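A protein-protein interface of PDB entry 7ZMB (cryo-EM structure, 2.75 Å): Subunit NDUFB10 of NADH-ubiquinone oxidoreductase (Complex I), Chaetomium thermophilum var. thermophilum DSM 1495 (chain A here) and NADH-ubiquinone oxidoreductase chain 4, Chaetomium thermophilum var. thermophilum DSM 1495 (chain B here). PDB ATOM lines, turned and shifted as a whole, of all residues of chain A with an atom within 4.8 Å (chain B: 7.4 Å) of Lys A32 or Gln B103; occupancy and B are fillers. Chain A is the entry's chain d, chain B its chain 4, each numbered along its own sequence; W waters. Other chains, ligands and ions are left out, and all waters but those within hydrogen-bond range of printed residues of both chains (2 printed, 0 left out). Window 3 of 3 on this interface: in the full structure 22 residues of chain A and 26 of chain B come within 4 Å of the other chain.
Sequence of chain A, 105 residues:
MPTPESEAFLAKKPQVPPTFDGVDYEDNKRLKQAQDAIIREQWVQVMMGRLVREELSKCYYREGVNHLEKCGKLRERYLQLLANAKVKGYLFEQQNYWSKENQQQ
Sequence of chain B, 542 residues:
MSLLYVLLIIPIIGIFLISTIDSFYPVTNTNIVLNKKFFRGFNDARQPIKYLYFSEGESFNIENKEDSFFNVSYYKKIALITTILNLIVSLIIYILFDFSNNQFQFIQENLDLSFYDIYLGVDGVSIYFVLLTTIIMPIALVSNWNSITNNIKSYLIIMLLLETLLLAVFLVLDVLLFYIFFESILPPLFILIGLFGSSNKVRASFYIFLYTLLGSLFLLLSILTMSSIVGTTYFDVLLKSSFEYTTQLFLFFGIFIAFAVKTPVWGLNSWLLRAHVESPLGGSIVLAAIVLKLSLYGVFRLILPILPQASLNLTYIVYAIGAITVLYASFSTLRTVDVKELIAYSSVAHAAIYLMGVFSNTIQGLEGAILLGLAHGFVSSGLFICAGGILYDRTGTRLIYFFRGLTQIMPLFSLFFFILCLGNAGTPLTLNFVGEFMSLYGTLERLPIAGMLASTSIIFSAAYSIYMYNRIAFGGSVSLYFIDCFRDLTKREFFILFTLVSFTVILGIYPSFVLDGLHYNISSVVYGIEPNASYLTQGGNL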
ATOM      1  N   ASN A  28      27.383 -21.888  -6.461  1.00  0.00           N
ATOM      2  CA  ASN A  28      27.539 -22.901  -5.422  1.00  0.00           C
ATOM      3  C   ASN A  28      26.199 -23.499  -5.013  1.00  0.00           C
ATOM      4  O   ASN A  28      26.110 -24.699  -4.740  1.00  0.00           O
ATOM      5  CB  ASN A  28      28.261 -22.300  -4.218  1.00  0.00           C
ATOM      6  CG  ASN A  28      29.748 -22.147  -4.455  1.00  0.00           C
ATOM      7  OD1 ASN A  28      30.435 -23.109  -4.798  1.00  0.00           O
ATOM      8  ND2 ASN A  28      30.251 -20.929  -4.294  1.00  0.00           N
ATOM      9  N   LYS A  29      25.149 -22.677  -4.964  1.00  0.00           N
ATOM     10  CA  LYS A  29      23.820 -23.174  -4.616  1.00  0.00           C
ATOM     11  C   LYS A  29      23.349 -24.248  -5.583  1.00  0.00           C
ATOM     12  O   LYS A  29      22.694 -25.212  -5.171  1.00  0.00           O
ATOM     13  CB  LYS A  29      22.826 -22.010  -4.582  1.00  0.00           C
ATOM     14  CG  LYS A  29      21.386 -22.402  -4.269  1.00  0.00           C
ATOM     15  CD  LYS A  29      20.518 -21.170  -4.052  1.00  0.00           C
ATOM     16  CE  LYS A  29      20.133 -20.504  -5.362  1.00  0.00           C
ATOM     17  NZ  LYS A  29      19.113 -21.285  -6.113  1.00  0.00           N
ATOM     18  N   ARG A  30      23.685 -24.103  -6.865  1.00  0.00           N
ATOM     19  CA  ARG A  30      23.274 -25.052  -7.893  1.00  0.00           C
ATOM     20  C   ARG A  30      24.092 -26.336  -7.865  1.00  0.00           C
ATOM     21  O   ARG A  30      23.534 -27.432  -7.969  1.00  0.00           O
ATOM     22  CB  ARG A  30      23.373 -24.388  -9.261  1.00  0.00           C
ATOM     23  CG  ARG A  30      22.715 -25.157 -10.352  1.00  0.00           C
ATOM     24  CD  ARG A  30      21.220 -25.289 -10.204  1.00  0.00           C
ATOM     25  NE  ARG A  30      20.763 -26.410 -11.021  1.00  0.00           N
ATOM     26  CZ  ARG A  30      21.151 -27.672 -10.857  1.00  0.00           C
ATOM     27  NH1 ARG A  30      21.951 -28.011  -9.860  1.00  0.00           N
ATOM     28  NH2 ARG A  30      20.710 -28.611 -11.676  1.00  0.00           N
ATOM     29  N   LEU A  31      25.415 -26.221  -7.733  1.00  0.00           N
ATOM     30  CA  LEU A  31      26.261 -27.410  -7.736  1.00  0.00           C
ATOM     31  C   LEU A  31      25.871 -28.365  -6.621  1.00  0.00           C
ATOM     32  O   LEU A  31      25.843 -29.583  -6.814  1.00  0.00           O
ATOM     33  CB  LEU A  31      27.728 -27.012  -7.602  1.00  0.00           C
ATOM     34  CG  LEU A  31      28.704 -28.181  -7.660  1.00  0.00           C
ATOM     35  CD1 LEU A  31      28.615 -28.859  -9.002  1.00  0.00           C
ATOM     36  CD2 LEU A  31      30.112 -27.738  -7.379  1.00  0.00           C
ATOM     37  N   LYS A  32      25.559 -27.825  -5.450  1.00  0.00           N
ATOM     38  CA  LYS A  32      25.203 -28.662  -4.315  1.00  0.00           C
ATOM     39  C   LYS A  32      23.875 -29.374  -4.543  1.00  0.00           C
ATOM     40  O   LYS A  32      23.747 -30.572  -4.267  1.00  0.00           O
ATOM     41  CB  LYS A  32      25.163 -27.808  -3.056  1.00  0.00           C
ATOM     42  CG  LYS A  32      26.500 -27.196  -2.716  1.00  0.00           C
ATOM     43  CD  LYS A  32      27.459 -28.230  -2.175  1.00  0.00           C
ATOM     44  CE  LYS A  32      27.360 -28.331  -0.668  1.00  0.00           C
ATOM     45  NZ  LYS A  32      27.986 -29.569  -0.153  1.00  0.00           N
ATOM     46  N   GLN A  33      22.879 -28.656  -5.066  1.00  0.00           N
ATOM     47  CA  GLN A  33      21.583 -29.270  -5.325  1.00  0.00           C
ATOM     48  C   GLN A  33      21.697 -30.398  -6.331  1.00  0.00           C
ATOM     49  O   GLN A  33      21.042 -31.436  -6.185  1.00  0.00           O
ATOM     50  CB  GLN A  33      20.597 -28.226  -5.830  1.00  0.00           C
ATOM     51  CG  GLN A  33      19.923 -27.455  -4.745  1.00  0.00           C
ATOM     52  CD  GLN A  33      19.564 -26.069  -5.181  1.00  0.00           C
ATOM     53  OE1 GLN A  33      19.951 -25.632  -6.259  1.00  0.00           O
ATOM     54  NE2 GLN A  33      18.817 -25.362  -4.348  1.00  0.00           N
ATOM     55  N   ALA A  34      22.505 -30.200  -7.376  1.00  0.00           N
ATOM     56  CA  ALA A  34      22.748 -31.257  -8.348  1.00  0.00           C
ATOM     57  C   ALA A  34      23.374 -32.471  -7.684  1.00  0.00           C
ATOM     58  O   ALA A  34      22.938 -33.604  -7.901  1.00  0.00           O
ATOM     59  CB  ALA A  34      23.645 -30.741  -9.466  1.00  0.00           C
ATOM     60  N   GLN A  35      24.396 -32.248  -6.854  1.00  0.00           N
ATOM     61  CA  GLN A  35      24.985 -33.352  -6.105  1.00  0.00           C
ATOM     62  C   GLN A  35      23.943 -34.018  -5.225  1.00  0.00           C
ATOM     63  O   GLN A  35      23.845 -35.249  -5.193  1.00  0.00           O
ATOM     64  CB  GLN A  35      26.152 -32.863  -5.251  1.00  0.00           C
ATOM     65  CG  GLN A  35      27.296 -32.259  -6.013  1.00  0.00           C
ATOM     66  CD  GLN A  35      28.147 -31.365  -5.151  1.00  0.00           C
ATOM     67  OE1 GLN A  35      27.683 -30.831  -4.154  1.00  0.00           O
ATOM     68  NE2 GLN A  35      29.402 -31.190  -5.534  1.00  0.00           N
ATOM     69  N   ASP A  36      23.142 -33.217  -4.519  1.00  0.00           N
ATOM     70  CA  ASP A  36      22.115 -33.778  -3.650  1.00  0.00           C
ATOM     71  C   ASP A  36      21.130 -34.623  -4.433  1.00  0.00           C
ATOM     72  O   ASP A  36      20.866 -35.774  -4.076  1.00  0.00           O
ATOM     73  CB  ASP A  36      21.357 -32.679  -2.925  1.00  0.00           C
ATOM     74  CG  ASP A  36      20.104 -33.195  -2.267  1.00  0.00           C
ATOM     75  OD1 ASP A  36      20.193 -34.228  -1.576  1.00  0.00           O
ATOM     76  OD2 ASP A  36      19.028 -32.586  -2.456  1.00  0.00           O
ATOM     77  N   PHE B  97      21.718 -31.852  14.847  1.00  0.00           N
ATOM     78  CA  PHE B  97      22.332 -32.224  13.552  1.00  0.00           C
ATOM     79  C   PHE B  97      21.326 -32.877  12.615  1.00  0.00           C
ATOM     80  O   PHE B  97      20.509 -33.689  13.064  1.00  0.00           O
ATOM     81  CB  PHE B  97      23.583 -33.080  13.768  1.00  0.00           C
ATOM     82  CG  PHE B  97      24.322 -33.445  12.508  1.00  0.00           C
ATOM     83  CD1 PHE B  97      25.041 -32.492  11.808  1.00  0.00           C
ATOM     84  CD2 PHE B  97      24.307 -34.743  12.028  1.00  0.00           C
ATOM     85  CE1 PHE B  97      25.718 -32.829  10.650  1.00  0.00           C
ATOM     86  CE2 PHE B  97      24.983 -35.079  10.867  1.00  0.00           C
ATOM     87  CZ  PHE B  97      25.684 -34.120  10.180  1.00  0.00           C
ATOM     88  N   ASP B  98      21.413 -32.544  11.338  1.00  0.00           N
ATOM     89  CA  ASP B  98      20.559 -33.106  10.302  1.00  0.00           C
ATOM     90  C   ASP B  98      21.356 -34.124   9.496  1.00  0.00           C
ATOM     91  O   ASP B  98      22.440 -33.812   8.993  1.00  0.00           O
ATOM     92  CB  ASP B  98      20.025 -31.984   9.408  1.00  0.00           C
ATOM     93  CG  ASP B  98      19.251 -32.492   8.215  1.00  0.00           C
ATOM     94  OD1 ASP B  98      18.637 -33.570   8.301  1.00  0.00           O
ATOM     95  OD2 ASP B  98      19.241 -31.798   7.184  1.00  0.00           O
ATOM     96  N   SER B 100      20.752 -35.653   6.657  1.00  0.00           N
ATOM     97  CA  SER B 100      20.497 -35.781   5.230  1.00  0.00           C
ATOM     98  C   SER B 100      20.810 -34.488   4.494  1.00  0.00           C
ATOM     99  O   SER B 100      20.199 -34.189   3.466  1.00  0.00           O
ATOM    100  CB  SER B 100      19.053 -36.201   4.978  1.00  0.00           C
ATOM    101  OG  SER B 100      18.736 -37.375   5.694  1.00  0.00           O
ATOM    102  N   ASN B 101      21.758 -33.694   5.014  1.00  0.00           N
ATOM    103  CA  ASN B 101      22.110 -32.385   4.384  1.00  0.00           C
ATOM    104  C   ASN B 101      23.566 -32.343   3.897  1.00  0.00           C
ATOM    105  O   ASN B 101      24.457 -32.628   4.703  1.00  0.00           O
ATOM    106  CB  ASN B 101      21.833 -31.219   5.333  1.00  0.00           C
ATOM    107  CG  ASN B 101      22.121 -29.857   4.743  1.00  0.00           C
ATOM    108  OD1 ASN B 101      22.060 -29.669   3.531  1.00  0.00           O
ATOM    109  ND2 ASN B 101      22.416 -28.895   5.600  1.00  0.00           N
ATOM    110  N   ASN B 102      23.793 -32.009   2.620  1.00  0.00           N
ATOM    111  CA  ASN B 102      25.167 -31.880   2.054  1.00  0.00           C
ATOM    112  C   ASN B 102      25.915 -30.659   2.608  1.00  0.00           C
ATOM    113  O   ASN B 102      27.114 -30.789   2.880  1.00  0.00           O
ATOM    114  CB  ASN B 102      25.207 -32.049   0.529  1.00  0.00           C
ATOM    115  CG  ASN B 102      24.562 -30.939  -0.266  1.00  0.00           C
ATOM    116  OD1 ASN B 102      23.937 -30.037   0.286  1.00  0.00           O
ATOM    117  ND2 ASN B 102      24.705 -31.006  -1.578  1.00  0.00           N
ATOM    118  N   GLN B 103      25.236 -29.532   2.793  1.00  0.00           N
ATOM    119  CA  GLN B 103      25.882 -28.275   3.248  1.00  0.00           C
ATOM    120  C   GLN B 103      26.529 -28.478   4.619  1.00  0.00           C
ATOM    121  O   GLN B 103      25.913 -29.152   5.458  1.00  0.00           O
ATOM    122  CB  GLN B 103      24.788 -27.221   3.427  1.00  0.00           C
ATOM    123  CG  GLN B 103      23.898 -27.042   2.209  1.00  0.00           C
ATOM    124  CD  GLN B 103      24.603 -26.335   1.079  1.00  0.00           C
ATOM    125  OE1 GLN B 103      25.547 -25.579   1.287  1.00  0.00           O
ATOM    126  NE2 GLN B 103      24.137 -26.567  -0.135  1.00  0.00           N
ATOM    127  N   PHE B 104      27.706 -27.901   4.860  1.00  0.00           N
ATOM    128  CA  PHE B 104      28.281 -28.012   6.229  1.00  0.00           C
ATOM    129  C   PHE B 104      27.367 -27.269   7.213  1.00  0.00           C
ATOM    130  O   PHE B 104      26.893 -26.167   6.881  1.00  0.00           O
ATOM    131  CB  PHE B 104      29.732 -27.525   6.270  1.00  0.00           C
ATOM    132  CG  PHE B 104      30.752 -28.417   5.616  1.00  0.00           C
ATOM    133  CD1 PHE B 104      31.165 -29.588   6.230  1.00  0.00           C
ATOM    134  CD2 PHE B 104      31.324 -28.068   4.408  1.00  0.00           C
ATOM    135  CE1 PHE B 104      32.114 -30.400   5.632  1.00  0.00           C
ATOM    136  CE2 PHE B 104      32.272 -28.882   3.811  1.00  0.00           C
ATOM    137  CZ  PHE B 104      32.666 -30.047   4.425  1.00  0.00           C
ATOM    138  N   GLN B 105      27.110 -27.854   8.387  1.00  0.00           N
ATOM    139  CA  GLN B 105      26.142 -27.235   9.339  1.00  0.00           C
ATOM    140  C   GLN B 105      26.859 -26.517  10.484  1.00  0.00           C
ATOM    141  O   GLN B 105      28.022 -26.866  10.742  1.00  0.00           O
ATOM    142  CB  GLN B 105      25.169 -28.288   9.863  1.00  0.00           C
ATOM    143  CG  GLN B 105      24.371 -28.987   8.775  1.00  0.00           C
ATOM    144  CD  GLN B 105      23.568 -30.134   9.335  1.00  0.00           C
ATOM    145  OE1 GLN B 105      23.134 -30.109  10.482  1.00  0.00           O
ATOM    146  NE2 GLN B 105      23.366 -31.154   8.520  1.00  0.00           N
ATOM    147  N   PHE B 106      26.191 -25.566  11.140  1.00  0.00           N
ATOM    148  CA  PHE B 106      26.743 -24.802  12.259  1.00  0.00           C
ATOM    149  C   PHE B 106      27.979 -24.011  11.841  1.00  0.00           C
ATOM    150  O   PHE B 106      28.975 -23.946  12.560  1.00  0.00           O
ATOM    151  CB  PHE B 106      27.026 -25.703  13.457  1.00  0.00           C
ATOM    152  CG  PHE B 106      25.863 -26.550  13.841  1.00  0.00           C
ATOM    153  CD1 PHE B 106      24.756 -25.988  14.437  1.00  0.00           C
ATOM    154  CD2 PHE B 106      25.860 -27.905  13.572  1.00  0.00           C
ATOM    155  CE1 PHE B 106      23.670 -26.763  14.774  1.00  0.00           C
ATOM    156  CE2 PHE B 106      24.781 -28.680  13.902  1.00  0.00           C
ATOM    157  CZ  PHE B 106      23.683 -28.107  14.509  1.00  0.00           C
ATOM    158  N   ILE B 107      27.901 -23.405  10.675  1.00  0.00           N
ATOM    159  CA  ILE B 107      28.901 -22.472  10.179  1.00  0.00           C
ATOM    160  C   ILE B 107      28.531 -21.078  10.646  1.00  0.00           C
ATOM    161  O   ILE B 107      27.380 -20.802  10.993  1.00  0.00           O
ATOM    162  CB  ILE B 107      28.996 -22.526   8.646  1.00  0.00           C
ATOM    163  CG1 ILE B 107      27.656 -22.110   8.051  1.00  0.00           C
ATOM    164  CG2 ILE B 107      29.402 -23.911   8.184  1.00  0.00           C
ATOM    165  CD1 ILE B 107      27.696 -21.893   6.586  1.00  0.00           C
ATOM    166  N   VAL B 122      30.353 -28.751  10.551  1.00  0.00           N
ATOM    167  CA  VAL B 122      30.006 -30.110  11.056  1.00  0.00           C
ATOM    168  C   VAL B 122      29.120 -30.799  10.022  1.00  0.00           C
ATOM    169  O   VAL B 122      28.007 -30.310   9.774  1.00  0.00           O
ATOM    170  CB  VAL B 122      29.331 -30.055  12.442  1.00  0.00           C
ATOM    171  CG1 VAL B 122      28.424 -31.249  12.690  1.00  0.00           C
ATOM    172  CG2 VAL B 122      30.346 -29.947  13.561  1.00  0.00           C
ATOM    173  N   ASP B 123      29.631 -31.843   9.378  1.00  0.00           N
ATOM    174  CA  ASP B 123      28.786 -32.646   8.454  1.00  0.00           C
ATOM    175  C   ASP B 123      28.706 -34.060   9.014  1.00  0.00           C
ATOM    176  O   ASP B 123      29.030 -34.230  10.203  1.00  0.00           O
ATOM    177  CB  ASP B 123      29.302 -32.668   7.019  1.00  0.00           C
ATOM    178  CG  ASP B 123      30.616 -33.405   6.845  1.00  0.00           C
ATOM    179  OD1 ASP B 123      31.314 -33.604   7.855  1.00  0.00           O
ATOM    180  OD2 ASP B 123      30.925 -33.780   5.698  1.00  0.00           O
ATOM    181  N   GLY B 124      28.329 -35.035   8.190  1.00  0.00           N
ATOM    182  CA  GLY B 124      28.133 -36.385   8.679  1.00  0.00           C
ATOM    183  C   GLY B 124      29.397 -37.100   9.088  1.00  0.00           C
ATOM    184  O   GLY B 124      29.420 -37.761  10.128  1.00  0.00           O
ATOM    185  N   ASP B 236      34.684 -26.368   0.261  1.00  0.00           N
ATOM    186  CA  ASP B 236      33.673 -26.234  -0.781  1.00  0.00           C
ATOM    187  C   ASP B 236      34.287 -25.866  -2.122  1.00  0.00           C
ATOM    188  O   ASP B 236      33.911 -26.430  -3.151  1.00  0.00           O
ATOM    189  CB  ASP B 236      32.629 -25.204  -0.362  1.00  0.00           C
ATOM    190  CG  ASP B 236      31.625 -25.772   0.620  1.00  0.00           C
ATOM    191  OD1 ASP B 236      31.565 -27.012   0.749  1.00  0.00           O
ATOM    192  OD2 ASP B 236      30.897 -24.985   1.261  1.00  0.00           O
ATOM    193  N   LEU B 239      37.002 -29.023  -3.236  1.00  0.00           N
ATOM    194  CA  LEU B 239      36.490 -30.346  -3.577  1.00  0.00           C
ATOM    195  C   LEU B 239      36.080 -30.433  -5.043  1.00  0.00           C
ATOM    196  O   LEU B 239      36.341 -31.442  -5.709  1.00  0.00           O
ATOM    197  CB  LEU B 239      35.308 -30.692  -2.676  1.00  0.00           C
ATOM    198  CG  LEU B 239      35.638 -31.024  -1.224  1.00  0.00           C
ATOM    199  CD1 LEU B 239      34.446 -31.637  -0.527  1.00  0.00           C
ATOM    200  CD2 LEU B 239      36.852 -31.916  -1.143  1.00  0.00           C
ATOM    201  N   TYR B 520      24.221 -40.347   4.243  1.00  0.00           N
ATOM    202  CA  TYR B 520      24.087 -39.383   3.159  1.00  0.00           C
ATOM    203  C   TYR B 520      25.411 -38.695   2.852  1.00  0.00           C
ATOM    204  O   TYR B 520      25.782 -38.543   1.681  1.00  0.00           O
ATOM    205  CB  TYR B 520      23.010 -38.366   3.524  1.00  0.00           C
ATOM    206  CG  TYR B 520      22.757 -37.294   2.496  1.00  0.00           C
ATOM    207  CD1 TYR B 520      21.951 -37.535   1.396  1.00  0.00           C
ATOM    208  CD2 TYR B 520      23.314 -36.040   2.635  1.00  0.00           C
ATOM    209  CE1 TYR B 520      21.717 -36.558   0.467  1.00  0.00           C
ATOM    210  CE2 TYR B 520      23.086 -35.059   1.709  1.00  0.00           C
ATOM    211  CZ  TYR B 520      22.286 -35.318   0.634  1.00  0.00           C
ATOM    212  OH  TYR B 520      22.065 -34.330  -0.285  1.00  0.00           O
ATOM    213  N   ASN B 521      26.148 -38.287   3.880  1.00  0.00           N
ATOM    214  CA  ASN B 521      27.402 -37.583   3.640  1.00  0.00           C
ATOM    215  C   ASN B 521      28.516 -38.499   3.166  1.00  0.00           C
ATOM    216  O   ASN B 521      29.437 -38.033   2.488  1.00  0.00           O
ATOM    217  CB  ASN B 521      27.842 -36.828   4.893  1.00  0.00           C
ATOM    218  CG  ASN B 521      26.877 -35.736   5.273  1.00  0.00           C
ATOM    219  OD1 ASN B 521      26.235 -35.788   6.317  1.00  0.00           O
ATOM    220  ND2 ASN B 521      26.771 -34.730   4.422  1.00  0.00           N
HETATM  221  O   HOH W   1      21.767 -27.128  -2.180  1.00  0.00           O
HETATM  222  O   HOH W   2      22.013 -30.037  -1.588  1.00  0.00           O
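Water W2 lies within hydrogen-bond range of the side-chain amide oxygen (OD1) of Asn B102 (2.7 Å) and the backbone carbonyl oxygen (O) of Lys A32 (3.2 Å). Water W1 lies within hydrogen-bond range of NE2 of Gln B103 and N of Gln A33.
Lys A32 touches just these residues of chain B: Asn B102 and Gln B103. Of chain A, only Lys A32 (3.3 Å) comes within 4 Å of Gln B103. Printed residues of chain A within 4 Å of Tyr B520: Asp A36 (2.3 Å). Of the printed residues of chain B, Asp A36 touches Asn B102 (3.98 Å) and Tyr B520 (2.3 Å). The nearest residue of chain B that does not touch Lys A32 is Asp B236 (4.5 Å). The nearest printed residue of chain B that does not touch Asp A36 is Ser B100 (5.0 Å).
The side-chain carboxylate (OD1) of Asp A36 sits close to the side-chain hydroxyl (OH) of Tyr B520, 2.3 Å away. O of Lys A32 lies within hydrogen-bond range of ND2 of Asn B102 (2.9 Å).
Hydrophobic or aromatic side chains of chain B that line the printed part of chain A: Tyr B520. Of the 9 printed residues of chain A, 3 touch a printed residue of chain B. Among the printed residues, no Asp or Glu carboxylate lies within 4 Å of a Lys or Arg side-chain nitrogen of the other chain.
Among the printed residues, merely in contact across the chains: Lys A32 with Gln B103, Gln A35 with Asn B102 and Asp A36 with Asn B102.
OD1 of Asn B101 is in hydrogen-bond range of N of Gln B103 (3.3 Å). O of Leu A31 lies close to OE1 of Gln A35, at 3.5 Å.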
